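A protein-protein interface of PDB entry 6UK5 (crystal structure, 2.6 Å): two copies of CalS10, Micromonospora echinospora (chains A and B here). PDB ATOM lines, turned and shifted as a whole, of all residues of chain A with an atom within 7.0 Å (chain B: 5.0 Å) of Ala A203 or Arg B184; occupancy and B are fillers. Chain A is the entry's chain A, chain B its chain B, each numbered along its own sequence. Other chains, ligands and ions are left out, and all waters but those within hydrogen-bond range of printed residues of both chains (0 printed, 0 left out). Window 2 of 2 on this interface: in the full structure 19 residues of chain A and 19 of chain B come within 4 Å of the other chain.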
ATOM      1  N   GLY A 176      -5.833  10.181  24.052  1.00  0.00           N
ATOM      2  CA  GLY A 176      -4.395  10.076  23.954  1.00  0.00           C
ATOM      3  C   GLY A 176      -3.734  11.122  23.078  1.00  0.00           C
ATOM      4  O   GLY A 176      -2.500  11.220  23.092  1.00  0.00           O
ATOM      5  N   ARG A 177      -4.500  11.896  22.313  1.00  0.00           N
ATOM      6  CA  ARG A 177      -3.929  13.006  21.559  1.00  0.00           C
ATOM      7  C   ARG A 177      -5.045  13.966  21.170  1.00  0.00           C
ATOM      8  O   ARG A 177      -6.192  13.558  20.971  1.00  0.00           O
ATOM      9  CB  ARG A 177      -3.155  12.539  20.324  1.00  0.00           C
ATOM     10  CG  ARG A 177      -3.987  11.878  19.260  1.00  0.00           C
ATOM     11  CD  ARG A 177      -3.203  11.807  17.973  1.00  0.00           C
ATOM     12  NE  ARG A 177      -4.044  11.469  16.836  1.00  0.00           N
ATOM     13  CZ  ARG A 177      -3.609  11.414  15.583  1.00  0.00           C
ATOM     14  NH1 ARG A 177      -2.337  11.676  15.310  1.00  0.00           N
ATOM     15  NH2 ARG A 177      -4.443  11.098  14.606  1.00  0.00           N
ATOM     16  N   GLY A 201      -0.875  17.619  20.458  1.00  0.00           N
ATOM     17  CA  GLY A 201      -0.512  17.423  21.850  1.00  0.00           C
ATOM     18  C   GLY A 201      -0.920  16.023  22.278  1.00  0.00           C
ATOM     19  O   GLY A 201      -2.042  15.587  22.015  1.00  0.00           O
ATOM     20  N   ASP A 202       0.002  15.329  22.933  1.00  0.00           N
ATOM     21  CA  ASP A 202      -0.237  13.942  23.306  1.00  0.00           C
ATOM     22  C   ASP A 202       0.609  13.620  24.535  1.00  0.00           C
ATOM     23  O   ASP A 202       1.102  14.524  25.219  1.00  0.00           O
ATOM     24  CB  ASP A 202       0.065  13.016  22.113  1.00  0.00           C
ATOM     25  CG  ASP A 202       1.455  13.234  21.542  1.00  0.00           C
ATOM     26  OD1 ASP A 202       2.339  13.704  22.291  1.00  0.00           O
ATOM     27  OD2 ASP A 202       1.663  12.925  20.349  1.00  0.00           O
ATOM     28  N   ALA A 203       0.775  12.326  24.815  1.00  0.00           N
ATOM     29  CA  ALA A 203       1.554  11.904  25.973  1.00  0.00           C
ATOM     30  C   ALA A 203       2.946  12.519  25.950  1.00  0.00           C
ATOM     31  O   ALA A 203       3.457  12.960  26.987  1.00  0.00           O
ATOM     32  CB  ALA A 203       1.646  10.376  26.005  1.00  0.00           C
ATOM     33  N   ALA A 204       3.575  12.557  24.774  1.00  0.00           N
ATOM     34  CA  ALA A 204       4.971  12.962  24.678  1.00  0.00           C
ATOM     35  C   ALA A 204       5.174  14.471  24.770  1.00  0.00           C
ATOM     36  O   ALA A 204       6.228  14.916  25.239  1.00  0.00           O
ATOM     37  CB  ALA A 204       5.566  12.449  23.365  1.00  0.00           C
ATOM     38  N   GLY A 205       4.207  15.269  24.350  1.00  0.00           N
ATOM     39  CA  GLY A 205       4.366  16.708  24.370  1.00  0.00           C
ATOM     40  C   GLY A 205       3.485  17.365  23.327  1.00  0.00           C
ATOM     41  O   GLY A 205       2.570  16.753  22.783  1.00  0.00           O
ATOM     42  N   ILE A 206       3.775  18.640  23.071  1.00  0.00           N
ATOM     43  CA  ILE A 206       3.094  19.427  22.048  1.00  0.00           C
ATOM     44  C   ILE A 206       4.025  19.553  20.849  1.00  0.00           C
ATOM     45  O   ILE A 206       5.128  20.100  20.970  1.00  0.00           O
ATOM     46  CB  ILE A 206       2.706  20.821  22.570  1.00  0.00           C
ATOM     47  CG1 ILE A 206       1.796  20.734  23.797  1.00  0.00           C
ATOM     48  CG2 ILE A 206       2.042  21.624  21.460  1.00  0.00           C
ATOM     49  CD1 ILE A 206       1.549  22.081  24.474  1.00  0.00           C
ATOM     50  N   GLY B 165       0.711  15.595  32.560  1.00  0.00           N
ATOM     51  CA  GLY B 165       0.674  15.442  31.125  1.00  0.00           C
ATOM     52  C   GLY B 165      -0.696  15.702  30.553  1.00  0.00           C
ATOM     53  O   GLY B 165      -1.010  15.212  29.466  1.00  0.00           O
ATOM     54  N   TYR B 166      -1.534  16.451  31.269  1.00  0.00           N
ATOM     55  CA  TYR B 166      -2.879  16.715  30.781  1.00  0.00           C
ATOM     56  C   TYR B 166      -2.787  17.603  29.549  1.00  0.00           C
ATOM     57  O   TYR B 166      -2.040  18.585  29.529  1.00  0.00           O
ATOM     58  CB  TYR B 166      -3.744  17.387  31.843  1.00  0.00           C
ATOM     59  CG  TYR B 166      -5.139  17.668  31.332  1.00  0.00           C
ATOM     60  CD1 TYR B 166      -6.063  16.638  31.225  1.00  0.00           C
ATOM     61  CD2 TYR B 166      -5.527  18.941  30.940  1.00  0.00           C
ATOM     62  CE1 TYR B 166      -7.337  16.865  30.755  1.00  0.00           C
ATOM     63  CE2 TYR B 166      -6.805  19.180  30.464  1.00  0.00           C
ATOM     64  CZ  TYR B 166      -7.705  18.136  30.373  1.00  0.00           C
ATOM     65  OH  TYR B 166      -8.979  18.355  29.904  1.00  0.00           O
ATOM     66  N   VAL B 167      -3.557  17.262  28.524  1.00  0.00           N
ATOM     67  CA  VAL B 167      -3.531  17.975  27.256  1.00  0.00           C
ATOM     68  C   VAL B 167      -4.914  18.551  26.990  1.00  0.00           C
ATOM     69  O   VAL B 167      -5.896  17.804  26.888  1.00  0.00           O
ATOM     70  CB  VAL B 167      -3.087  17.046  26.114  1.00  0.00           C
ATOM     71  CG1 VAL B 167      -3.331  17.698  24.788  1.00  0.00           C
ATOM     72  CG2 VAL B 167      -1.619  16.678  26.258  1.00  0.00           C
ATOM     73  N   GLY B 168      -4.991  19.878  26.874  1.00  0.00           N
ATOM     74  CA  GLY B 168      -6.238  20.545  26.547  1.00  0.00           C
ATOM     75  C   GLY B 168      -6.247  21.188  25.173  1.00  0.00           C
ATOM     76  O   GLY B 168      -5.188  21.419  24.583  1.00  0.00           O
ATOM     77  N   VAL B 182      -3.739  24.479  21.797  1.00  0.00           N
ATOM     78  CA  VAL B 182      -3.438  23.203  22.435  1.00  0.00           C
ATOM     79  C   VAL B 182      -2.540  23.479  23.629  1.00  0.00           C
ATOM     80  O   VAL B 182      -1.559  24.222  23.514  1.00  0.00           O
ATOM     81  CB  VAL B 182      -2.774  22.213  21.462  1.00  0.00           C
ATOM     82  CG1 VAL B 182      -2.362  20.954  22.197  1.00  0.00           C
ATOM     83  CG2 VAL B 182      -3.732  21.874  20.329  1.00  0.00           C
ATOM     84  N   SER B 183      -2.880  22.894  24.771  1.00  0.00           N
ATOM     85  CA  SER B 183      -2.141  23.101  26.005  1.00  0.00           C
ATOM     86  C   SER B 183      -1.642  21.767  26.546  1.00  0.00           C
ATOM     87  O   SER B 183      -2.137  20.696  26.185  1.00  0.00           O
ATOM     88  CB  SER B 183      -3.009  23.802  27.058  1.00  0.00           C
ATOM     89  OG  SER B 183      -4.074  22.965  27.470  1.00  0.00           O
ATOM     90  N   ARG B 184      -0.635  21.852  27.411  1.00  0.00           N
ATOM     91  CA  ARG B 184      -0.078  20.681  28.076  1.00  0.00           C
ATOM     92  C   ARG B 184       0.396  21.125  29.446  1.00  0.00           C
ATOM     93  O   ARG B 184       1.081  22.147  29.560  1.00  0.00           O
ATOM     94  CB  ARG B 184       1.086  20.056  27.302  1.00  0.00           C
ATOM     95  CG  ARG B 184       1.465  18.664  27.823  1.00  0.00           C
ATOM     96  CD  ARG B 184       2.592  18.032  27.012  1.00  0.00           C
ATOM     97  NE  ARG B 184       2.878  16.656  27.424  1.00  0.00           N
ATOM     98  CZ  ARG B 184       3.926  16.238  28.132  1.00  0.00           C
ATOM     99  NH1 ARG B 184       4.881  17.070  28.526  1.00  0.00           N
ATOM    100  NH2 ARG B 184       4.026  14.949  28.424  1.00  0.00           N
ATOM    101  N   SER B 185       0.033  20.371  30.477  1.00  0.00           N
ATOM    102  CA  SER B 185       0.414  20.702  31.841  1.00  0.00           C
ATOM    103  C   SER B 185       1.267  19.576  32.404  1.00  0.00           C
ATOM    104  O   SER B 185       0.867  18.407  32.377  1.00  0.00           O
ATOM    105  CB  SER B 185      -0.826  20.922  32.709  1.00  0.00           C
ATOM    106  OG  SER B 185      -1.803  21.671  32.005  1.00  0.00           O
ATOM    107  N   THR B 186       2.444  19.941  32.903  1.00  0.00           N
ATOM    108  CA  THR B 186       3.355  19.020  33.560  1.00  0.00           C
ATOM    109  C   THR B 186       3.819  19.618  34.878  1.00  0.00           C
ATOM    110  O   THR B 186       3.814  20.836  35.072  1.00  0.00           O
ATOM    111  CB  THR B 186       4.579  18.696  32.694  1.00  0.00           C
ATOM    112  OG1 THR B 186       5.307  19.898  32.416  1.00  0.00           O
ATOM    113  CG2 THR B 186       4.156  18.042  31.399  1.00  0.00           C
ATOM    114  N   ARG B 193       3.774  23.259  35.194  1.00  0.00           N
ATOM    115  CA  ARG B 193       4.176  23.876  33.939  1.00  0.00           C
ATOM    116  C   ARG B 193       3.060  23.723  32.913  1.00  0.00           C
ATOM    117  O   ARG B 193       2.843  22.626  32.390  1.00  0.00           O
ATOM    118  CB  ARG B 193       5.470  23.244  33.433  1.00  0.00           C
ATOM    119  CG  ARG B 193       6.100  23.992  32.280  1.00  0.00           C
ATOM    120  CD  ARG B 193       7.421  23.371  31.884  1.00  0.00           C
ATOM    121  NE  ARG B 193       7.946  23.962  30.658  1.00  0.00           N
ATOM    122  CZ  ARG B 193       7.519  23.677  29.432  1.00  0.00           C
ATOM    123  NH1 ARG B 193       6.543  22.799  29.242  1.00  0.00           N
ATOM    124  NH2 ARG B 193       8.075  24.282  28.392  1.00  0.00           N
ATOM    125  N   MET B 194       2.359  24.818  32.626  1.00  0.00           N
ATOM    126  CA  MET B 194       1.322  24.832  31.603  1.00  0.00           C
ATOM    127  C   MET B 194       1.940  25.403  30.332  1.00  0.00           C
ATOM    128  O   MET B 194       2.384  26.557  30.319  1.00  0.00           O
ATOM    129  CB  MET B 194       0.100  25.653  32.014  1.00  0.00           C
ATOM    130  CG  MET B 194      -1.072  25.458  31.051  1.00  0.00           C
ATOM    131  SD  MET B 194      -2.486  26.533  31.351  1.00  0.00           S
ATOM    132  CE  MET B 194      -3.807  25.484  30.738  1.00  0.00           C
ATOM    133  N   GLU B 195       1.963  24.604  29.272  1.00  0.00           N
ATOM    134  CA  GLU B 195       2.475  25.028  27.976  1.00  0.00           C
ATOM    135  C   GLU B 195       1.286  25.252  27.054  1.00  0.00           C
ATOM    136  O   GLU B 195       0.526  24.320  26.776  1.00  0.00           O
ATOM    137  CB  GLU B 195       3.425  23.980  27.399  1.00  0.00           C
ATOM    138  CG  GLU B 195       4.203  24.438  26.177  1.00  0.00           C
ATOM    139  CD  GLU B 195       4.905  23.298  25.479  1.00  0.00           C
ATOM    140  OE1 GLU B 195       5.248  23.467  24.289  1.00  0.00           O
ATOM    141  OE2 GLU B 195       5.101  22.238  26.116  1.00  0.00           O
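Among the printed residues, merely in contact across the chains: Gly A201 with Val B167 (3.7 Å), Asp A202 with Val B167 (3.6 Å), Asp A202 with Arg B184 (3.5 Å), Ala A204 with Arg B184 (3.9 Å), Gly A205 with Arg B184 (3.4 Å), Ile A206 with Val B182 (3.9 Å), Ile A206 with Ser B183 (3.8 Å), Ile A206 with Arg B184 (3.5 Å) and Ile A206 with Glu B195 (3.4 Å).
No position is printed for both chains.
The guanidinium group (NH1) of Arg B193 is in salt-bridge range of the side-chain carboxylate (OE2) of Glu B195, at 3.5 Å.
N of Gly A205 is in hydrogen-bond range of OD1 of Asp A202 (3.2 Å).
The backbone carbonyl oxygen (O) of Gly B168 sits at hydrogen-bond distance from the backbone NH (N) of Ser B183, at 2.7 Å.
The backbone NH of Glu B195 is in hydrogen-bond range of the backbone carbonyl oxygen of Arg B184 (2.6 Å).
The side-chain carboxylate (OD1) of Asp A202 is in hydrogen-bond range of the backbone NH (N) of Ala A204 (3.0 Å).
The backbone carbonyl oxygen (O) of Ala A203 lies within hydrogen-bond range of the guanidinium group (NH2) of Arg B184, 2.5 Å away.
Gly A176 touches none of the printed residues of chain B.
Ala A203 touches just one residue of chain B: Arg B184 (2.5 Å).
Printed residues of chain B within 4 Å of Gly A205: Arg B184.
Printed residues of chain B within 4 Å of Ile A206: Val B182 (3.9 Å), Ser B183 (3.8 Å), Arg B184 (3.5 Å) and Glu B195 (3.4 Å).
Printed residues of chain A within 4 Å of Val B182: Ile A206.
Of chain A, only Asp A202 (3.5 Å), Ala A203 (2.5 Å), Ala A204 (3.9 Å), Gly A205 (3.4 Å) and Ile A206 (3.5 Å) come within 4 Å of Arg B184.
Printed residues of chain A within 4 Å of Glu B195: Ile A206 (3.4 Å).
The nearest printed residue of chain B that does not touch Ala A203 is Val B167 (5.2 Å).
The nearest residue of chain A that does not touch Arg B184 is Gly A201 (6.1 Å).
Of the 8 printed residues of chain A, 6 touch a printed residue of chain B.
Of the 12 printed residues of chain B, 5 touch a printed residue of chain A.
Hydrophobic or aromatic side chains of chain B that line the printed part of chain A: Val B167.
Among the printed residues, 10 pairs touch across the chains.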
